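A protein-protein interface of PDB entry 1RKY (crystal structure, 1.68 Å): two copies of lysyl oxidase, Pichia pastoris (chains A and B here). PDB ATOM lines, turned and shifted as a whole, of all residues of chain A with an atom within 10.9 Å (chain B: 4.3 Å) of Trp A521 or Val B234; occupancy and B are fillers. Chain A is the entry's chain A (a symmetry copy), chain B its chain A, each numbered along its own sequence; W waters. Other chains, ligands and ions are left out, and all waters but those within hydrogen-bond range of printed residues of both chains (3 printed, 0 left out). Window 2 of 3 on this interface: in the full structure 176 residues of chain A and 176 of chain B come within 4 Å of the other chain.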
ATOM      1  N   VAL A 517       3.427 -18.599   5.387  1.00  0.00           N
ATOM      2  CA  VAL A 517       2.204 -17.896   5.021  1.00  0.00           C
ATOM      3  C   VAL A 517       2.373 -16.416   5.333  1.00  0.00           C
ATOM      4  O   VAL A 517       3.269 -16.012   6.084  1.00  0.00           O
ATOM      5  CB  VAL A 517       0.958 -18.439   5.798  1.00  0.00           C
ATOM      6  CG1 VAL A 517       0.793 -19.956   5.602  1.00  0.00           C
ATOM      7  CG2 VAL A 517       1.047 -18.131   7.266  1.00  0.00           C
ATOM      8  N   GLU A 518       1.502 -15.621   4.730  1.00  0.00           N
ATOM      9  CA  GLU A 518       1.301 -14.236   5.101  1.00  0.00           C
ATOM     10  C   GLU A 518      -0.155 -14.128   5.443  1.00  0.00           C
ATOM     11  O   GLU A 518      -1.005 -14.755   4.797  1.00  0.00           O
ATOM     12  CB  GLU A 518       1.615 -13.309   3.918  1.00  0.00           C
ATOM     13  CG  GLU A 518       3.087 -12.985   3.738  1.00  0.00           C
ATOM     14  CD  GLU A 518       3.321 -11.979   2.619  1.00  0.00           C
ATOM     15  OE1 GLU A 518       2.641 -10.932   2.611  1.00  0.00           O
ATOM     16  OE2 GLU A 518       4.173 -12.233   1.741  1.00  0.00           O
ATOM     17  N   TYR A 519      -0.458 -13.313   6.433  1.00  0.00           N
ATOM     18  CA  TYR A 519      -1.795 -13.118   6.896  1.00  0.00           C
ATOM     19  C   TYR A 519      -2.334 -11.742   6.498  1.00  0.00           C
ATOM     20  O   TYR A 519      -1.559 -10.791   6.434  1.00  0.00           O
ATOM     21  CB  TYR A 519      -1.839 -13.210   8.410  1.00  0.00           C
ATOM     22  CG  TYR A 519      -1.489 -14.599   8.937  1.00  0.00           C
ATOM     23  CD1 TYR A 519      -0.266 -14.838   9.540  1.00  0.00           C
ATOM     24  CD2 TYR A 519      -2.400 -15.643   8.830  1.00  0.00           C
ATOM     25  CE1 TYR A 519       0.049 -16.087  10.031  1.00  0.00           C
ATOM     26  CE2 TYR A 519      -2.080 -16.921   9.328  1.00  0.00           C
ATOM     27  CZ  TYR A 519      -0.861 -17.112   9.922  1.00  0.00           C
ATOM     28  OH  TYR A 519      -0.538 -18.353  10.440  1.00  0.00           O
ATOM     29  N   PRO A 520      -3.645 -11.636   6.280  1.00  0.00           N
ATOM     30  CA  PRO A 520      -4.243 -10.329   5.917  1.00  0.00           C
ATOM     31  C   PRO A 520      -4.085  -9.265   7.009  1.00  0.00           C
ATOM     32  O   PRO A 520      -4.069  -8.072   6.694  1.00  0.00           O
ATOM     33  CB  PRO A 520      -5.728 -10.659   5.664  1.00  0.00           C
ATOM     34  CG  PRO A 520      -5.965 -12.017   6.281  1.00  0.00           C
ATOM     35  CD  PRO A 520      -4.639 -12.725   6.277  1.00  0.00           C
ATOM     36  N   TRP A 521      -3.948  -9.691   8.265  1.00  0.00           N
ATOM     37  CA  TRP A 521      -3.752  -8.780   9.388  1.00  0.00           C
ATOM     38  C   TRP A 521      -2.293  -8.381   9.668  1.00  0.00           C
ATOM     39  O   TRP A 521      -2.055  -7.561  10.544  1.00  0.00           O
ATOM     40  CB  TRP A 521      -4.460  -9.305  10.654  1.00  0.00           C
ATOM     41  CG  TRP A 521      -4.215 -10.776  10.966  1.00  0.00           C
ATOM     42  CD1 TRP A 521      -5.071 -11.805  10.760  1.00  0.00           C
ATOM     43  CD2 TRP A 521      -3.041 -11.337  11.540  1.00  0.00           C
ATOM     44  NE1 TRP A 521      -4.496 -12.991  11.163  1.00  0.00           N
ATOM     45  CE2 TRP A 521      -3.246 -12.733  11.644  1.00  0.00           C
ATOM     46  CE3 TRP A 521      -1.825 -10.808  11.975  1.00  0.00           C
ATOM     47  CZ2 TRP A 521      -2.277 -13.606  12.182  1.00  0.00           C
ATOM     48  CZ3 TRP A 521      -0.846 -11.680  12.485  1.00  0.00           C
ATOM     49  CH2 TRP A 521      -1.094 -13.065  12.588  1.00  0.00           C
ATOM     50  N   ALA A 522      -1.330  -8.918   8.924  1.00  0.00           N
ATOM     51  CA  ALA A 522       0.075  -8.467   9.003  1.00  0.00           C
ATOM     52  C   ALA A 522       0.769  -8.533   7.652  1.00  0.00           C
ATOM     53  O   ALA A 522       1.671  -9.357   7.429  1.00  0.00           O
ATOM     54  CB  ALA A 522       0.875  -9.280  10.059  1.00  0.00           C
ATOM     55  N   PRO A 523       0.390  -7.621   6.745  1.00  0.00           N
ATOM     56  CA  PRO A 523       0.865  -7.686   5.369  1.00  0.00           C
ATOM     57  C   PRO A 523       2.373  -7.578   5.324  1.00  0.00           C
ATOM     58  O   PRO A 523       2.957  -6.775   6.061  1.00  0.00           O
ATOM     59  CB  PRO A 523       0.203  -6.465   4.703  1.00  0.00           C
ATOM     60  CG  PRO A 523      -0.919  -6.091   5.606  1.00  0.00           C
ATOM     61  CD  PRO A 523      -0.476  -6.452   6.981  1.00  0.00           C
ATOM     62  N   GLY A 524       3.001  -8.418   4.503  1.00  0.00           N
ATOM     63  CA  GLY A 524       4.430  -8.356   4.286  1.00  0.00           C
ATOM     64  C   GLY A 524       5.253  -9.124   5.306  1.00  0.00           C
ATOM     65  O   GLY A 524       6.472  -9.184   5.201  1.00  0.00           O
ATOM     66  N   THR A 525       4.594  -9.708   6.300  1.00  0.00           N
ATOM     67  CA  THR A 525       5.291 -10.476   7.322  1.00  0.00           C
ATOM     68  C   THR A 525       5.078 -11.969   7.085  1.00  0.00           C
ATOM     69  O   THR A 525       3.951 -12.440   7.152  1.00  0.00           O
ATOM     70  CB  THR A 525       4.769 -10.081   8.717  1.00  0.00           C
ATOM     71  OG1 THR A 525       5.025  -8.689   8.956  1.00  0.00           O
ATOM     72  CG2 THR A 525       5.554 -10.780   9.829  1.00  0.00           C
ATOM     73  N   VAL A 526       6.163 -12.696   6.835  1.00  0.00           N
ATOM     74  CA  VAL A 526       6.091 -14.144   6.610  1.00  0.00           C
ATOM     75  C   VAL A 526       6.180 -14.855   7.966  1.00  0.00           C
ATOM     76  O   VAL A 526       7.041 -14.541   8.781  1.00  0.00           O
ATOM     77  CB  VAL A 526       7.177 -14.643   5.706  1.00  0.00           C
ATOM     78  CG1 VAL A 526       7.034 -16.152   5.476  1.00  0.00           C
ATOM     79  CG2 VAL A 526       7.114 -13.914   4.370  1.00  0.00           C
ATOM     80  N   TYR A 527       5.254 -15.784   8.178  1.00  0.00           N
ATOM     81  CA  TYR A 527       5.216 -16.640   9.360  1.00  0.00           C
ATOM     82  C   TYR A 527       5.463 -18.071   8.889  1.00  0.00           C
ATOM     83  O   TYR A 527       4.935 -18.489   7.876  1.00  0.00           O
ATOM     84  CB  TYR A 527       3.842 -16.601   9.998  1.00  0.00           C
ATOM     85  CG  TYR A 527       3.597 -15.399  10.856  1.00  0.00           C
ATOM     86  CD1 TYR A 527       3.266 -14.171  10.296  1.00  0.00           C
ATOM     87  CD2 TYR A 527       3.647 -15.493  12.233  1.00  0.00           C
ATOM     88  CE1 TYR A 527       3.024 -13.062  11.101  1.00  0.00           C
ATOM     89  CE2 TYR A 527       3.405 -14.376  13.057  1.00  0.00           C
ATOM     90  CZ  TYR A 527       3.098 -13.162  12.471  1.00  0.00           C
ATOM     91  OH  TYR A 527       2.865 -12.063  13.276  1.00  0.00           O
ATOM     92  N   ASN A 528       6.270 -18.815   9.621  1.00  0.00           N
ATOM     93  CA  ASN A 528       6.348 -20.262   9.432  1.00  0.00           C
ATOM     94  C   ASN A 528       5.373 -20.849  10.447  1.00  0.00           C
ATOM     95  O   ASN A 528       5.553 -20.687  11.640  1.00  0.00           O
ATOM     96  CB  ASN A 528       7.782 -20.753   9.685  1.00  0.00           C
ATOM     97  CG  ASN A 528       7.946 -22.253   9.531  1.00  0.00           C
ATOM     98  OD1 ASN A 528       8.495 -22.914  10.426  1.00  0.00           O
ATOM     99  ND2 ASN A 528       7.549 -22.792   8.389  1.00  0.00           N
ATOM    100  N   THR A 529       4.320 -21.472   9.945  1.00  0.00           N
ATOM    101  CA  THR A 529       3.294 -22.025  10.783  1.00  0.00           C
ATOM    102  C   THR A 529       2.997 -23.458  10.343  1.00  0.00           C
ATOM    103  O   THR A 529       3.816 -24.076   9.711  1.00  0.00           O
ATOM    104  CB  THR A 529       2.077 -21.118  10.769  1.00  0.00           C
ATOM    105  OG1 THR A 529       1.123 -21.580  11.733  1.00  0.00           O
ATOM    106  CG2 THR A 529       1.354 -21.115   9.424  1.00  0.00           C
ATOM    107  N   TYR B 190      -0.555  -9.247  21.330  1.00  0.00           N
ATOM    108  CA  TYR B 190      -1.870  -9.384  20.751  1.00  0.00           C
ATOM    109  C   TYR B 190      -2.772  -9.872  21.851  1.00  0.00           C
ATOM    110  O   TYR B 190      -2.311 -10.279  22.924  1.00  0.00           O
ATOM    111  CB  TYR B 190      -1.851 -10.366  19.564  1.00  0.00           C
ATOM    112  CG  TYR B 190      -1.173  -9.853  18.303  1.00  0.00           C
ATOM    113  CD1 TYR B 190       0.218  -9.965  18.112  1.00  0.00           C
ATOM    114  CD2 TYR B 190      -1.920  -9.284  17.280  1.00  0.00           C
ATOM    115  CE1 TYR B 190       0.838  -9.502  16.948  1.00  0.00           C
ATOM    116  CE2 TYR B 190      -1.308  -8.835  16.120  1.00  0.00           C
ATOM    117  CZ  TYR B 190       0.047  -8.925  15.956  1.00  0.00           C
ATOM    118  OH  TYR B 190       0.586  -8.481  14.767  1.00  0.00           O
ATOM    119  N   GLU B 227      -3.922  -1.741  17.085  1.00  0.00           N
ATOM    120  CA  GLU B 227      -4.863  -2.286  16.111  1.00  0.00           C
ATOM    121  C   GLU B 227      -6.037  -2.963  16.772  1.00  0.00           C
ATOM    122  O   GLU B 227      -5.927  -3.521  17.873  1.00  0.00           O
ATOM    123  CB  GLU B 227      -4.181  -3.315  15.198  1.00  0.00           C
ATOM    124  CG  GLU B 227      -2.967  -2.815  14.472  1.00  0.00           C
ATOM    125  CD  GLU B 227      -2.248  -3.895  13.698  1.00  0.00           C
ATOM    126  OE1 GLU B 227      -1.451  -3.555  12.791  1.00  0.00           O
ATOM    127  OE2 GLU B 227      -2.467  -5.090  13.990  1.00  0.00           O
ATOM    128  N   TYR B 228      -7.172  -2.908  16.086  1.00  0.00           N
ATOM    129  CA  TYR B 228      -8.294  -3.802  16.320  1.00  0.00           C
ATOM    130  C   TYR B 228      -8.414  -4.630  15.071  1.00  0.00           C
ATOM    131  O   TYR B 228      -8.287  -4.104  13.963  1.00  0.00           O
ATOM    132  CB  TYR B 228      -9.575  -3.026  16.592  1.00  0.00           C
ATOM    133  CG  TYR B 228      -9.517  -2.281  17.905  1.00  0.00           C
ATOM    134  CD1 TYR B 228      -9.565  -0.889  17.960  1.00  0.00           C
ATOM    135  CD2 TYR B 228      -9.396  -2.973  19.097  1.00  0.00           C
ATOM    136  CE1 TYR B 228      -9.482  -0.226  19.173  1.00  0.00           C
ATOM    137  CE2 TYR B 228      -9.316  -2.324  20.308  1.00  0.00           C
ATOM    138  CZ  TYR B 228      -9.355  -0.955  20.345  1.00  0.00           C
ATOM    139  OH  TYR B 228      -9.279  -0.348  21.577  1.00  0.00           O
ATOM    140  N   ILE B 229      -8.586  -5.942  15.235  1.00  0.00           N
ATOM    141  CA  ILE B 229      -8.644  -6.857  14.109  1.00  0.00           C
ATOM    142  C   ILE B 229      -9.926  -7.664  14.208  1.00  0.00           C
ATOM    143  O   ILE B 229     -10.230  -8.256  15.236  1.00  0.00           O
ATOM    144  CB  ILE B 229      -7.388  -7.774  14.071  1.00  0.00           C
ATOM    145  CG1 ILE B 229      -6.120  -6.921  13.954  1.00  0.00           C
ATOM    146  CG2 ILE B 229      -7.496  -8.773  12.918  1.00  0.00           C
ATOM    147  CD1 ILE B 229      -4.841  -7.636  14.377  1.00  0.00           C
ATOM    148  N   ASN B 232     -10.615 -10.441   9.723  1.00  0.00           N
ATOM    149  CA  ASN B 232      -9.394 -10.318   8.934  1.00  0.00           C
ATOM    150  C   ASN B 232      -9.092  -8.917   8.382  1.00  0.00           C
ATOM    151  O   ASN B 232      -8.270  -8.757   7.468  1.00  0.00           O
ATOM    152  CB  ASN B 232      -9.360 -11.356   7.809  1.00  0.00           C
ATOM    153  CG  ASN B 232      -9.134 -12.748   8.349  1.00  0.00           C
ATOM    154  OD1 ASN B 232      -8.106 -13.004   8.994  1.00  0.00           O
ATOM    155  ND2 ASN B 232     -10.107 -13.632   8.142  1.00  0.00           N
ATOM    156  N   LYS B 233      -9.725  -7.924   8.980  1.00  0.00           N
ATOM    157  CA  LYS B 233      -9.475  -6.509   8.650  1.00  0.00           C
ATOM    158  C   LYS B 233      -8.857  -5.773   9.842  1.00  0.00           C
ATOM    159  O   LYS B 233      -9.242  -6.002  10.972  1.00  0.00           O
ATOM    160  CB  LYS B 233     -10.782  -5.842   8.252  1.00  0.00           C
ATOM    161  CG  LYS B 233     -11.485  -6.539   7.096  1.00  0.00           C
ATOM    162  CD  LYS B 233     -12.642  -5.715   6.532  1.00  0.00           C
ATOM    163  CE  LYS B 233     -13.361  -6.487   5.429  1.00  0.00           C
ATOM    164  NZ  LYS B 233     -12.550  -6.521   4.179  1.00  0.00           N
ATOM    165  N   VAL B 234      -7.919  -4.874   9.561  1.00  0.00           N
ATOM    166  CA  VAL B 234      -7.192  -4.122  10.579  1.00  0.00           C
ATOM    167  C   VAL B 234      -7.733  -2.680  10.626  1.00  0.00           C
ATOM    168  O   VAL B 234      -7.845  -2.021   9.572  1.00  0.00           O
ATOM    169  CB  VAL B 234      -5.698  -4.083  10.241  1.00  0.00           C
ATOM    170  CG1 VAL B 234      -4.899  -3.459  11.351  1.00  0.00           C
ATOM    171  CG2 VAL B 234      -5.168  -5.501   9.944  1.00  0.00           C
ATOM    172  N   TYR B 235      -8.070  -2.236  11.838  1.00  0.00           N
ATOM    173  CA  TYR B 235      -8.511  -0.866  12.152  1.00  0.00           C
ATOM    174  C   TYR B 235      -7.487  -0.211  13.081  1.00  0.00           C
ATOM    175  O   TYR B 235      -7.011  -0.840  14.014  1.00  0.00           O
ATOM    176  CB  TYR B 235      -9.889  -0.908  12.808  1.00  0.00           C
ATOM    177  CG  TYR B 235     -10.906  -1.630  11.955  1.00  0.00           C
ATOM    178  CD1 TYR B 235     -11.029  -3.019  12.000  1.00  0.00           C
ATOM    179  CD2 TYR B 235     -11.716  -0.930  11.060  1.00  0.00           C
ATOM    180  CE1 TYR B 235     -11.942  -3.689  11.195  1.00  0.00           C
ATOM    181  CE2 TYR B 235     -12.627  -1.591  10.226  1.00  0.00           C
ATOM    182  CZ  TYR B 235     -12.741  -2.971  10.305  1.00  0.00           C
ATOM    183  OH  TYR B 235     -13.649  -3.632   9.516  1.00  0.00           O
ATOM    184  N   ASP B 347      -5.240 -19.125  11.747  1.00  0.00           N
ATOM    185  CA  ASP B 347      -5.474 -17.999  10.847  1.00  0.00           C
ATOM    186  C   ASP B 347      -5.584 -16.689  11.620  1.00  0.00           C
ATOM    187  O   ASP B 347      -5.480 -15.607  11.007  1.00  0.00           O
ATOM    188  CB  ASP B 347      -6.747 -18.222  10.023  1.00  0.00           C
ATOM    189  CG  ASP B 347      -8.000 -18.414  10.871  1.00  0.00           C
ATOM    190  OD1 ASP B 347      -7.978 -19.119  11.922  1.00  0.00           O
ATOM    191  OD2 ASP B 347      -9.086 -17.901  10.537  1.00  0.00           O
ATOM    192  N   ASP B 348      -5.825 -16.770  12.928  1.00  0.00           N
ATOM    193  CA  ASP B 348      -6.045 -15.572  13.740  1.00  0.00           C
ATOM    194  C   ASP B 348      -4.816 -15.140  14.565  1.00  0.00           C
ATOM    195  O   ASP B 348      -3.926 -15.939  14.850  1.00  0.00           O
ATOM    196  CB  ASP B 348      -7.351 -15.697  14.547  1.00  0.00           C
ATOM    197  CG  ASP B 348      -7.199 -16.443  15.886  1.00  0.00           C
ATOM    198  OD1 ASP B 348      -8.046 -17.304  16.191  1.00  0.00           O
ATOM    199  OD2 ASP B 348      -6.352 -16.156  16.728  1.00  0.00           O
ATOM    200  N   PRO B 349      -4.742 -13.848  14.899  1.00  0.00           N
ATOM    201  CA  PRO B 349      -3.561 -13.295  15.573  1.00  0.00           C
ATOM    202  C   PRO B 349      -3.398 -13.637  17.067  1.00  0.00           C
ATOM    203  O   PRO B 349      -2.345 -13.291  17.622  1.00  0.00           O
ATOM    204  CB  PRO B 349      -3.741 -11.779  15.398  1.00  0.00           C
ATOM    205  CG  PRO B 349      -5.194 -11.583  15.184  1.00  0.00           C
ATOM    206  CD  PRO B 349      -5.745 -12.813  14.576  1.00  0.00           C
ATOM    207  N   HIS B 353      -0.158 -16.490  17.683  1.00  0.00           N
ATOM    208  CA  HIS B 353       0.890 -15.973  18.542  1.00  0.00           C
ATOM    209  C   HIS B 353       0.958 -16.658  19.906  1.00  0.00           C
ATOM    210  O   HIS B 353       1.560 -16.116  20.837  1.00  0.00           O
ATOM    211  CB  HIS B 353       0.724 -14.474  18.719  1.00  0.00           C
ATOM    212  CG  HIS B 353       0.943 -13.718  17.458  1.00  0.00           C
ATOM    213  ND1 HIS B 353      -0.080 -13.097  16.777  1.00  0.00           N
ATOM    214  CD2 HIS B 353       2.068 -13.498  16.744  1.00  0.00           C
ATOM    215  CE1 HIS B 353       0.405 -12.543  15.680  1.00  0.00           C
ATOM    216  NE2 HIS B 353       1.706 -12.759  15.644  1.00  0.00           N
HETATM  217  O   HOH W   1      -0.965  -7.083  13.044  1.00  0.00           O
HETATM  218  O   HOH W   2       2.697  -9.390  13.220  1.00  0.00           O
HETATM  219  O   HOH W   3      -1.378  -4.879  10.423  1.00  0.00           O
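Of chain B, only Ile B229 (3.8 Å), Asn B232 (3.7 Å), Val B234 (3.6 Å), Asp B347 (2.8 Å), Asp B348 (3.8 Å), Pro B349 (3.6 Å) and His B353 (3.5 Å) come within 4 Å of Trp A521.
Val B234 touches one residue of chain A.
Asn B232 touches two residues of chain A.
No residue of chain A comes within 4 Å of Tyr B235.
Printed residues of chain A within 4 Å of Ile B229: Trp A521.
Of the printed residues of chain A, Asp B347 touches Tyr A519 and Trp A521.
Of the printed residues of chain B, Tyr A519 touches Asp B347 (3.8 Å).
Of the printed residues of chain B, Tyr A527 touches His B353 (2.7 Å).
Lys B233 touches none of the printed residues of chain A.
Tyr B190 touches none of the printed residues of chain A.
The nearest residue of chain B that does not touch Trp A521 is Tyr B190 (4.2 Å).
The indole nitrogen (NE1) of Trp A521 sits at hydrogen-bond distance from the backbone carbonyl oxygen (O) of Asp B347 (2.8 Å).
A ring nitrogen (NE2) of His B353 sits at hydrogen-bond distance from the side-chain hydroxyl (OH) of Tyr A527 (2.7 Å).
Printed residues of chain A that touch a printed residue of chain B: Tyr A519, Pro A520, Trp A521 and Tyr A527.
Hydrophobic or aromatic side chains of chain A that line the printed part of chain B: Tyr A519, Pro A520, Trp A521 and Tyr A527.
Hydrophobic or aromatic side chains of chain B that line the printed part of chain A: Ile B229, Val B234, Pro B349 and His B353.
Among the printed residues, no Asp or Glu carboxylate lies within 4 Å of a Lys or Arg side-chain nitrogen of the other chain.
Water W1 lies within hydrogen-bond range of the side-chain carboxylate (OE2) of Glu B227 (2.7 Å), the side-chain hydroxyl (OH) of Tyr B190 (2.7 Å) and the backbone carbonyl oxygen (O) of Trp A521 (2.8 Å).
Water W2 lies within hydrogen-bond range of the side-chain hydroxyl (OH) of Tyr A527 (2.7 Å) and the side-chain hydroxyl (OH) of Tyr B190 (2.8 Å).
Water W3 bridges the side-chain carboxylate of Glu B227 (2.7 Å) and the backbone carbonyl oxygen of Trp A521 (2.8 Å).
The backbone carbonyl oxygen (O) of Pro B349 lies within hydrogen-bond range of a ring nitrogen (ND1) of His B353.
The backbone carbonyl oxygen (O) of Val A517 is in hydrogen-bond range of the backbone NH (N) of Tyr A527 (2.9 Å).
No position is printed for both chains.
Among the printed residues, merely in contact across the chains: Tyr A519 with Asp B347, Pro A520 with Asn B232, Trp A521 with Ile B229, Trp A521 with Asn B232, Trp A521 with Val B234, Trp A521 with Asp B348, Trp A521 with Pro B349 and Trp A521 with His B353.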
